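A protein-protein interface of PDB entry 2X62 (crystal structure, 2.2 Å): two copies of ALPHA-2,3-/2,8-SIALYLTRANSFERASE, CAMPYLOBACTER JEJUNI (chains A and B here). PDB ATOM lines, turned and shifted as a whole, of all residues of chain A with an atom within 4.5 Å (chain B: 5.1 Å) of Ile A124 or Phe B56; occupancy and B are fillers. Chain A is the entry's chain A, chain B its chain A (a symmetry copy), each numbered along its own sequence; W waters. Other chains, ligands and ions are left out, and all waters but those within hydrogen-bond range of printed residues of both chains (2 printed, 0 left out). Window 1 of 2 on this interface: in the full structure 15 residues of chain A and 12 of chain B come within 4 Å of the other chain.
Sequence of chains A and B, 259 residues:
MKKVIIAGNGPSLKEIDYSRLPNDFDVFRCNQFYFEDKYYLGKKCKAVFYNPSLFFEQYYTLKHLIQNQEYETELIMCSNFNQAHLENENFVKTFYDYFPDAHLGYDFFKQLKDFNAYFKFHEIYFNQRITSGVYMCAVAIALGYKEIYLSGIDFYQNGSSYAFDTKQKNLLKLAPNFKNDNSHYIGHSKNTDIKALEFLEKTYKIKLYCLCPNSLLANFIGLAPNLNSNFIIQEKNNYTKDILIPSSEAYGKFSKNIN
The side-chain carboxylate (OE2) of Glu A123 lies within salt-bridge range of the side-chain amino group (NZ) of Lys B253 (2.9 Å).
OH of Tyr A125 lies within hydrogen-bond range of O of Phe B56, at 2.7 Å.
Among the printed residues, merely in contact across the chains: Gln A83 with Tyr B98, Lys A120 with Tyr B98, Ile A124 with Phe B56, Ile A124 with Tyr B98, Ile A124 with Ala B250, Ile A124 with Lys B253, Tyr A125 with Tyr B59, Tyr A125 with Tyr B60, Tyr A125 with Phe B99, Tyr A125 with Pro B246 and Phe A126 with Tyr B60.
Of chain B, only Phe B56, Tyr B98, Ala B250 and Lys B253 come within 4 Å of Ile A124.
Of the printed residues of chain A, Phe B56 touches Ile A124 (3.9 Å) and Tyr A125 (2.7 Å).
Of the printed residues of chain A, Lys B253 touches Glu A123 and Ile A124.
Of the printed residues of chain A, Pro B246 touches Tyr A125 (3.8 Å).
Of the printed residues of chain B, Glu A123 touches Lys B253 (2.8 Å).
Of the printed residues of chain B, Gln A83 touches Tyr B98.
Of the printed residues of chain A, Phe B99 touches Tyr A125.
The nearest printed residue of chain A that does not touch Phe B56 is Phe A121 (7.2 Å).
Of the 8 printed residues of chain A, 6 touch a printed residue of chain B.
Hydrophobic or aromatic side chains of chain B within 4 Å of the printed part of chain A: Phe B56, Tyr B59, Tyr B60, Tyr B98, Phe B99, Pro B246 and Ala B250.
Among the printed residues, Asp or Glu carboxylates within 4 Å of a Lys or Arg side-chain nitrogen of the other chain: Glu A123 with Lys B253 (2.9 Å).
No position is printed for both chains.
Of the 13 pairs that touch across the chains among the printed residues, none has its exchanged pair printed and touching as well.
Water W1 lies within hydrogen-bond range of O of Tyr A125 (2.6 Å) and OH of Tyr B60 (3.5 Å).
Water W2 bridges the backbone carbonyl oxygen (O) of Tyr B98 (2.9 Å) and the backbone NH (N) of Phe A121 (3.5 Å).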
ATOM      1  N   GLN A  83       3.236 -19.385  -5.643  1.00  0.00           N
ATOM      2  CA  GLN A  83       3.160 -17.964  -5.325  1.00  0.00           C
ATOM      3  C   GLN A  83       3.750 -17.704  -3.935  1.00  0.00           C
ATOM      4  O   GLN A  83       3.290 -18.230  -2.921  1.00  0.00           O
ATOM      5  CB  GLN A  83       1.703 -17.499  -5.360  1.00  0.00           C
ATOM      6  CG  GLN A  83       1.049 -17.522  -6.757  1.00  0.00           C
ATOM      7  CD  GLN A  83       1.437 -16.338  -7.636  1.00  0.00           C
ATOM      8  OE1 GLN A  83       0.818 -15.267  -7.572  1.00  0.00           O
ATOM      9  NE2 GLN A  83       2.446 -16.526  -8.466  1.00  0.00           N
ATOM     10  N   LYS A 120      -4.249 -16.649 -11.850  1.00  0.00           N
ATOM     11  CA  LYS A 120      -3.166 -15.772 -11.435  1.00  0.00           C
ATOM     12  C   LYS A 120      -3.539 -14.320 -11.673  1.00  0.00           C
ATOM     13  O   LYS A 120      -3.333 -13.458 -10.824  1.00  0.00           O
ATOM     14  CB  LYS A 120      -1.898 -16.138 -12.215  1.00  0.00           C
ATOM     15  CG  LYS A 120      -1.269 -17.491 -11.835  1.00  0.00           C
ATOM     16  CD  LYS A 120      -0.704 -17.453 -10.432  1.00  0.00           C
ATOM     17  CE  LYS A 120      -0.533 -18.865  -9.886  1.00  0.00           C
ATOM     18  NZ  LYS A 120       0.462 -19.686 -10.644  1.00  0.00           N
ATOM     19  N   PHE A 121      -4.136 -14.036 -12.813  1.00  0.00           N
ATOM     20  CA  PHE A 121      -4.487 -12.643 -13.137  1.00  0.00           C
ATOM     21  C   PHE A 121      -5.509 -12.100 -12.121  1.00  0.00           C
ATOM     22  O   PHE A 121      -5.362 -11.001 -11.583  1.00  0.00           O
ATOM     23  CB  PHE A 121      -4.965 -12.515 -14.593  1.00  0.00           C
ATOM     24  CG  PHE A 121      -5.376 -11.116 -14.989  1.00  0.00           C
ATOM     25  CD1 PHE A 121      -6.709 -10.809 -15.228  1.00  0.00           C
ATOM     26  CD2 PHE A 121      -4.439 -10.107 -15.110  1.00  0.00           C
ATOM     27  CE1 PHE A 121      -7.096  -9.518 -15.598  1.00  0.00           C
ATOM     28  CE2 PHE A 121      -4.820  -8.821 -15.462  1.00  0.00           C
ATOM     29  CZ  PHE A 121      -6.150  -8.532 -15.719  1.00  0.00           C
ATOM     30  N   HIS A 122      -6.512 -12.896 -11.801  1.00  0.00           N
ATOM     31  CA  HIS A 122      -7.487 -12.478 -10.825  1.00  0.00           C
ATOM     32  C   HIS A 122      -6.926 -12.358  -9.401  1.00  0.00           C
ATOM     33  O   HIS A 122      -7.242 -11.406  -8.705  1.00  0.00           O
ATOM     34  CB  HIS A 122      -8.653 -13.442 -10.866  1.00  0.00           C
ATOM     35  CG  HIS A 122      -9.478 -13.299 -12.098  1.00  0.00           C
ATOM     36  ND1 HIS A 122      -9.178 -13.952 -13.280  1.00  0.00           N
ATOM     37  CD2 HIS A 122     -10.558 -12.532 -12.354  1.00  0.00           C
ATOM     38  CE1 HIS A 122     -10.062 -13.609 -14.197  1.00  0.00           C
ATOM     39  NE2 HIS A 122     -10.911 -12.752 -13.659  1.00  0.00           N
ATOM     40  N   GLU A 123      -6.104 -13.310  -8.975  1.00  0.00           N
ATOM     41  CA  GLU A 123      -5.541 -13.278  -7.632  1.00  0.00           C
ATOM     42  C   GLU A 123      -4.587 -12.116  -7.455  1.00  0.00           C
ATOM     43  O   GLU A 123      -4.731 -11.336  -6.529  1.00  0.00           O
ATOM     44  CB  GLU A 123      -4.783 -14.581  -7.327  1.00  0.00           C
ATOM     45  CG  GLU A 123      -3.744 -14.434  -6.214  1.00  0.00           C
ATOM     46  CD  GLU A 123      -4.395 -14.047  -4.937  1.00  0.00           C
ATOM     47  OE1 GLU A 123      -5.604 -14.383  -4.829  1.00  0.00           O
ATOM     48  OE2 GLU A 123      -3.738 -13.427  -4.050  1.00  0.00           O
ATOM     49  N   ILE A 124      -3.606 -12.003  -8.351  1.00  0.00           N
ATOM     50  CA  ILE A 124      -2.541 -11.014  -8.215  1.00  0.00           C
ATOM     51  C   ILE A 124      -3.037  -9.582  -8.382  1.00  0.00           C
ATOM     52  O   ILE A 124      -2.652  -8.709  -7.615  1.00  0.00           O
ATOM     53  CB  ILE A 124      -1.421 -11.250  -9.249  1.00  0.00           C
ATOM     54  CG1 ILE A 124      -0.657 -12.532  -8.950  1.00  0.00           C
ATOM     55  CG2 ILE A 124      -0.426 -10.090  -9.281  1.00  0.00           C
ATOM     56  CD1 ILE A 124       0.126 -13.016 -10.150  1.00  0.00           C
ATOM     57  N   TYR A 125      -3.868  -9.343  -9.397  1.00  0.00           N
ATOM     58  CA  TYR A 125      -4.243  -7.992  -9.765  1.00  0.00           C
ATOM     59  C   TYR A 125      -5.558  -7.510  -9.138  1.00  0.00           C
ATOM     60  O   TYR A 125      -5.744  -6.313  -8.977  1.00  0.00           O
ATOM     61  CB  TYR A 125      -4.310  -7.839 -11.294  1.00  0.00           C
ATOM     62  CG  TYR A 125      -2.958  -7.869 -12.010  1.00  0.00           C
ATOM     63  CD1 TYR A 125      -2.521  -9.016 -12.627  1.00  0.00           C
ATOM     64  CD2 TYR A 125      -2.153  -6.739 -12.080  1.00  0.00           C
ATOM     65  CE1 TYR A 125      -1.316  -9.075 -13.265  1.00  0.00           C
ATOM     66  CE2 TYR A 125      -0.946  -6.776 -12.707  1.00  0.00           C
ATOM     67  CZ  TYR A 125      -0.533  -7.960 -13.318  1.00  0.00           C
ATOM     68  OH  TYR A 125       0.651  -8.038 -13.993  1.00  0.00           O
ATOM     69  N   PHE A 126      -6.458  -8.422  -8.786  1.00  0.00           N
ATOM     70  CA  PHE A 126      -7.780  -8.034  -8.264  1.00  0.00           C
ATOM     71  C   PHE A 126      -8.096  -8.652  -6.927  1.00  0.00           C
ATOM     72  O   PHE A 126      -9.196  -8.511  -6.411  1.00  0.00           O
ATOM     73  CB  PHE A 126      -8.883  -8.420  -9.253  1.00  0.00           C
ATOM     74  CG  PHE A 126      -8.806  -7.668 -10.532  1.00  0.00           C
ATOM     75  CD1 PHE A 126      -8.281  -8.250 -11.661  1.00  0.00           C
ATOM     76  CD2 PHE A 126      -9.185  -6.349 -10.584  1.00  0.00           C
ATOM     77  CE1 PHE A 126      -8.180  -7.538 -12.827  1.00  0.00           C
ATOM     78  CE2 PHE A 126      -9.077  -5.626 -11.763  1.00  0.00           C
ATOM     79  CZ  PHE A 126      -8.571  -6.222 -12.873  1.00  0.00           C
ATOM     80  N   PRO B  52      11.356  -6.157 -19.517  1.00  0.00           N
ATOM     81  CA  PRO B  52      11.212  -6.597 -18.142  1.00  0.00           C
ATOM     82  C   PRO B  52      10.828  -5.469 -17.166  1.00  0.00           C
ATOM     83  O   PRO B  52      10.056  -5.698 -16.222  1.00  0.00           O
ATOM     84  CB  PRO B  52      12.596  -7.144 -17.791  1.00  0.00           C
ATOM     85  CG  PRO B  52      13.318  -7.357 -19.070  1.00  0.00           C
ATOM     86  CD  PRO B  52      12.663  -6.501 -20.113  1.00  0.00           C
ATOM     87  N   LEU B  54       8.933  -2.754 -17.212  1.00  0.00           N
ATOM     88  CA  LEU B  54       7.516  -2.437 -16.969  1.00  0.00           C
ATOM     89  C   LEU B  54       6.552  -3.570 -17.274  1.00  0.00           C
ATOM     90  O   LEU B  54       5.394  -3.308 -17.645  1.00  0.00           O
ATOM     91  CB  LEU B  54       7.102  -1.216 -17.809  1.00  0.00           C
ATOM     92  CG  LEU B  54       7.776   0.084 -17.393  1.00  0.00           C
ATOM     93  CD1 LEU B  54       7.188   1.189 -18.184  1.00  0.00           C
ATOM     94  CD2 LEU B  54       7.599   0.325 -15.919  1.00  0.00           C
ATOM     95  N   PHE B  55       7.010  -4.815 -17.137  1.00  0.00           N
ATOM     96  CA  PHE B  55       6.221  -5.957 -17.596  1.00  0.00           C
ATOM     97  C   PHE B  55       4.970  -6.155 -16.759  1.00  0.00           C
ATOM     98  O   PHE B  55       3.907  -6.456 -17.300  1.00  0.00           O
ATOM     99  CB  PHE B  55       7.034  -7.267 -17.616  1.00  0.00           C
ATOM    100  CG  PHE B  55       6.298  -8.389 -18.278  1.00  0.00           C
ATOM    101  CD1 PHE B  55       6.412  -8.594 -19.625  1.00  0.00           C
ATOM    102  CD2 PHE B  55       5.441  -9.197 -17.548  1.00  0.00           C
ATOM    103  CE1 PHE B  55       5.703  -9.623 -20.248  1.00  0.00           C
ATOM    104  CE2 PHE B  55       4.724 -10.206 -18.155  1.00  0.00           C
ATOM    105  CZ  PHE B  55       4.845 -10.415 -19.516  1.00  0.00           C
ATOM    106  N   PHE B  56       5.091  -5.957 -15.444  1.00  0.00           N
ATOM    107  CA  PHE B  56       3.973  -6.120 -14.516  1.00  0.00           C
ATOM    108  C   PHE B  56       2.770  -5.250 -14.904  1.00  0.00           C
ATOM    109  O   PHE B  56       1.640  -5.731 -14.945  1.00  0.00           O
ATOM    110  CB  PHE B  56       4.446  -5.743 -13.121  1.00  0.00           C
ATOM    111  CG  PHE B  56       3.413  -5.900 -12.044  1.00  0.00           C
ATOM    112  CD1 PHE B  56       3.127  -4.847 -11.203  1.00  0.00           C
ATOM    113  CD2 PHE B  56       2.759  -7.102 -11.851  1.00  0.00           C
ATOM    114  CE1 PHE B  56       2.181  -4.967 -10.181  1.00  0.00           C
ATOM    115  CE2 PHE B  56       1.814  -7.252 -10.814  1.00  0.00           C
ATOM    116  CZ  PHE B  56       1.524  -6.188  -9.978  1.00  0.00           C
ATOM    117  N   GLU B  57       3.040  -3.974 -15.177  1.00  0.00           N
ATOM    118  CA  GLU B  57       2.045  -2.989 -15.562  1.00  0.00           C
ATOM    119  C   GLU B  57       1.588  -3.175 -17.022  1.00  0.00           C
ATOM    120  O   GLU B  57       0.419  -2.993 -17.331  1.00  0.00           O
ATOM    121  CB  GLU B  57       2.616  -1.568 -15.378  1.00  0.00           C
ATOM    122  CG  GLU B  57       2.893  -1.152 -13.929  1.00  0.00           C
ATOM    123  CD  GLU B  57       4.327  -1.441 -13.474  1.00  0.00           C
ATOM    124  OE1 GLU B  57       5.043  -2.207 -14.149  1.00  0.00           O
ATOM    125  OE2 GLU B  57       4.736  -0.889 -12.429  1.00  0.00           O
ATOM    126  N   GLN B  58       2.507  -3.543 -17.909  1.00  0.00           N
ATOM    127  CA  GLN B  58       2.160  -3.779 -19.320  1.00  0.00           C
ATOM    128  C   GLN B  58       1.261  -5.018 -19.489  1.00  0.00           C
ATOM    129  O   GLN B  58       0.399  -5.047 -20.374  1.00  0.00           O
ATOM    130  CB  GLN B  58       3.416  -3.955 -20.210  1.00  0.00           C
ATOM    131  CG  GLN B  58       4.287  -2.707 -20.385  1.00  0.00           C
ATOM    132  CD  GLN B  58       3.726  -1.679 -21.347  1.00  0.00           C
ATOM    133  OE1 GLN B  58       2.513  -1.506 -21.485  1.00  0.00           O
ATOM    134  NE2 GLN B  58       4.611  -1.001 -22.027  1.00  0.00           N
ATOM    135  N   TYR B  59       1.490  -6.045 -18.667  1.00  0.00           N
ATOM    136  CA  TYR B  59       0.656  -7.260 -18.709  1.00  0.00           C
ATOM    137  C   TYR B  59      -0.802  -6.960 -18.297  1.00  0.00           C
ATOM    138  O   TYR B  59      -1.758  -7.397 -18.951  1.00  0.00           O
ATOM    139  CB  TYR B  59       1.264  -8.358 -17.812  1.00  0.00           C
ATOM    140  CG  TYR B  59       0.547  -9.675 -17.896  1.00  0.00           C
ATOM    141  CD1 TYR B  59       0.850 -10.601 -18.891  1.00  0.00           C
ATOM    142  CD2 TYR B  59      -0.427 -10.008 -16.980  1.00  0.00           C
ATOM    143  CE1 TYR B  59       0.174 -11.820 -18.972  1.00  0.00           C
ATOM    144  CE2 TYR B  59      -1.088 -11.213 -17.046  1.00  0.00           C
ATOM    145  CZ  TYR B  59      -0.797 -12.111 -18.042  1.00  0.00           C
ATOM    146  OH  TYR B  59      -1.487 -13.305 -18.073  1.00  0.00           O
ATOM    147  N   TYR B  60      -0.934  -6.190 -17.223  1.00  0.00           N
ATOM    148  CA  TYR B  60      -2.209  -5.725 -16.693  1.00  0.00           C
ATOM    149  C   TYR B  60      -2.903  -4.879 -17.740  1.00  0.00           C
ATOM    150  O   TYR B  60      -4.099  -4.975 -17.933  1.00  0.00           O
ATOM    151  CB  TYR B  60      -1.930  -4.861 -15.462  1.00  0.00           C
ATOM    152  CG  TYR B  60      -3.112  -4.261 -14.757  1.00  0.00           C
ATOM    153  CD1 TYR B  60      -3.209  -2.889 -14.588  1.00  0.00           C
ATOM    154  CD2 TYR B  60      -4.096  -5.062 -14.190  1.00  0.00           C
ATOM    155  CE1 TYR B  60      -4.296  -2.316 -13.911  1.00  0.00           C
ATOM    156  CE2 TYR B  60      -5.178  -4.502 -13.502  1.00  0.00           C
ATOM    157  CZ  TYR B  60      -5.262  -3.131 -13.362  1.00  0.00           C
ATOM    158  OH  TYR B  60      -6.328  -2.573 -12.673  1.00  0.00           O
ATOM    159  N   TYR B  98       3.886 -16.498 -12.455  1.00  0.00           N
ATOM    160  CA  TYR B  98       3.145 -15.243 -12.326  1.00  0.00           C
ATOM    161  C   TYR B  98       2.368 -14.899 -13.592  1.00  0.00           C
ATOM    162  O   TYR B  98       1.327 -14.222 -13.512  1.00  0.00           O
ATOM    163  CB  TYR B  98       4.062 -14.079 -11.905  1.00  0.00           C
ATOM    164  CG  TYR B  98       4.366 -14.147 -10.432  1.00  0.00           C
ATOM    165  CD1 TYR B  98       5.328 -15.022  -9.945  1.00  0.00           C
ATOM    166  CD2 TYR B  98       3.613 -13.427  -9.529  1.00  0.00           C
ATOM    167  CE1 TYR B  98       5.570 -15.131  -8.585  1.00  0.00           C
ATOM    168  CE2 TYR B  98       3.834 -13.515  -8.190  1.00  0.00           C
ATOM    169  CZ  TYR B  98       4.819 -14.360  -7.719  1.00  0.00           C
ATOM    170  OH  TYR B  98       4.999 -14.462  -6.382  1.00  0.00           O
ATOM    171  N   PHE B  99       2.876 -15.374 -14.742  1.00  0.00           N
ATOM    172  CA  PHE B  99       2.291 -15.065 -16.036  1.00  0.00           C
ATOM    173  C   PHE B  99       2.175 -16.311 -16.901  1.00  0.00           C
ATOM    174  O   PHE B  99       2.910 -16.498 -17.857  1.00  0.00           O
ATOM    175  CB  PHE B  99       3.117 -13.996 -16.734  1.00  0.00           C
ATOM    176  CG  PHE B  99       3.401 -12.806 -15.864  1.00  0.00           C
ATOM    177  CD1 PHE B  99       4.636 -12.638 -15.295  1.00  0.00           C
ATOM    178  CD2 PHE B  99       2.419 -11.869 -15.616  1.00  0.00           C
ATOM    179  CE1 PHE B  99       4.881 -11.549 -14.476  1.00  0.00           C
ATOM    180  CE2 PHE B  99       2.658 -10.783 -14.842  1.00  0.00           C
ATOM    181  CZ  PHE B  99       3.892 -10.625 -14.254  1.00  0.00           C
ATOM    182  N   PRO B 246      -1.414  -0.878 -11.671  1.00  0.00           N
ATOM    183  CA  PRO B 246      -2.045  -1.823 -10.728  1.00  0.00           C
ATOM    184  C   PRO B 246      -2.210  -1.285  -9.299  1.00  0.00           C
ATOM    185  O   PRO B 246      -1.562  -0.292  -8.915  1.00  0.00           O
ATOM    186  CB  PRO B 246      -1.100  -3.025 -10.772  1.00  0.00           C
ATOM    187  CG  PRO B 246      -0.534  -3.001 -12.127  1.00  0.00           C
ATOM    188  CD  PRO B 246      -0.338  -1.521 -12.442  1.00  0.00           C
ATOM    189  N   GLU B 249      -2.146  -3.431  -3.502  1.00  0.00           N
ATOM    190  CA  GLU B 249      -2.238  -4.866  -3.189  1.00  0.00           C
ATOM    191  C   GLU B 249      -1.517  -5.695  -4.272  1.00  0.00           C
ATOM    192  O   GLU B 249      -0.712  -6.581  -3.972  1.00  0.00           O
ATOM    193  CB  GLU B 249      -3.721  -5.292  -3.077  1.00  0.00           C
ATOM    194  CG  GLU B 249      -4.514  -4.605  -1.938  1.00  0.00           C
ATOM    195  CD  GLU B 249      -5.048  -3.177  -2.246  1.00  0.00           C
ATOM    196  OE1 GLU B 249      -4.933  -2.664  -3.387  1.00  0.00           O
ATOM    197  OE2 GLU B 249      -5.614  -2.563  -1.309  1.00  0.00           O
ATOM    198  N   ALA B 250      -1.812  -5.426  -5.541  1.00  0.00           N
ATOM    199  CA  ALA B 250      -1.096  -6.109  -6.626  1.00  0.00           C
ATOM    200  C   ALA B 250       0.417  -5.935  -6.462  1.00  0.00           C
ATOM    201  O   ALA B 250       1.171  -6.893  -6.486  1.00  0.00           O
ATOM    202  CB  ALA B 250      -1.538  -5.584  -7.976  1.00  0.00           C
ATOM    203  N   TYR B 251       0.863  -4.699  -6.320  1.00  0.00           N
ATOM    204  CA  TYR B 251       2.291  -4.400  -6.170  1.00  0.00           C
ATOM    205  C   TYR B 251       2.912  -5.147  -4.996  1.00  0.00           C
ATOM    206  O   TYR B 251       4.008  -5.686  -5.112  1.00  0.00           O
ATOM    207  CB  TYR B 251       2.509  -2.897  -6.007  1.00  0.00           C
ATOM    208  CG  TYR B 251       2.603  -2.154  -7.335  1.00  0.00           C
ATOM    209  CD1 TYR B 251       3.801  -2.083  -8.026  1.00  0.00           C
ATOM    210  CD2 TYR B 251       1.496  -1.513  -7.892  1.00  0.00           C
ATOM    211  CE1 TYR B 251       3.908  -1.381  -9.259  1.00  0.00           C
ATOM    212  CE2 TYR B 251       1.590  -0.807  -9.121  1.00  0.00           C
ATOM    213  CZ  TYR B 251       2.798  -0.763  -9.797  1.00  0.00           C
ATOM    214  OH  TYR B 251       2.917  -0.074 -10.977  1.00  0.00           O
ATOM    215  N   LYS B 253       2.071  -7.922  -3.819  1.00  0.00           N
ATOM    216  CA  LYS B 253       2.260  -9.325  -4.149  1.00  0.00           C
ATOM    217  C   LYS B 253       3.389  -9.574  -5.165  1.00  0.00           C
ATOM    218  O   LYS B 253       3.898 -10.691  -5.275  1.00  0.00           O
ATOM    219  CB  LYS B 253       0.953  -9.915  -4.657  1.00  0.00           C
ATOM    220  CG  LYS B 253      -0.153  -9.990  -3.577  1.00  0.00           C
ATOM    221  CD  LYS B 253      -1.493 -10.334  -4.225  1.00  0.00           C
ATOM    222  CE  LYS B 253      -2.651 -10.237  -3.259  1.00  0.00           C
ATOM    223  NZ  LYS B 253      -3.917 -10.585  -3.922  1.00  0.00           N
ATOM    224  N   PHE B 254       3.794  -8.555  -5.903  1.00  0.00           N
ATOM    225  CA  PHE B 254       4.780  -8.762  -6.945  1.00  0.00           C
ATOM    226  C   PHE B 254       6.140  -8.191  -6.549  1.00  0.00           C
ATOM    227  O   PHE B 254       7.089  -8.231  -7.322  1.00  0.00           O
ATOM    228  CB  PHE B 254       4.302  -8.097  -8.228  1.00  0.00           C
ATOM    229  CG  PHE B 254       4.999  -8.589  -9.449  1.00  0.00           C
ATOM    230  CD1 PHE B 254       5.869  -7.768 -10.149  1.00  0.00           C
ATOM    231  CD2 PHE B 254       4.815  -9.892  -9.883  1.00  0.00           C
ATOM    232  CE1 PHE B 254       6.534  -8.237 -11.275  1.00  0.00           C
ATOM    233  CE2 PHE B 254       5.464 -10.365 -10.984  1.00  0.00           C
ATOM    234  CZ  PHE B 254       6.316  -9.533 -11.702  1.00  0.00           C
ATOM    235  N   ILE B 258      10.446  -6.799  -8.738  1.00  0.00           N
ATOM    236  CA  ILE B 258      10.611  -5.519  -9.431  1.00  0.00           C
ATOM    237  C   ILE B 258      11.894  -4.802  -9.009  1.00  0.00           C
ATOM    238  O   ILE B 258      12.623  -4.244  -9.854  1.00  0.00           O
ATOM    239  CB  ILE B 258       9.436  -4.565  -9.155  1.00  0.00           C
ATOM    240  CG1 ILE B 258       8.158  -5.068  -9.791  1.00  0.00           C
ATOM    241  CG2 ILE B 258       9.725  -3.190  -9.732  1.00  0.00           C
ATOM    242  CD1 ILE B 258       6.933  -4.299  -9.333  1.00  0.00           C
HETATM  243  O   HOH W   1      -4.744  -4.184 -10.010  1.00  0.00           O
HETATM  244  O   HOH W   2      -1.101 -12.725 -13.852  1.00  0.00           O
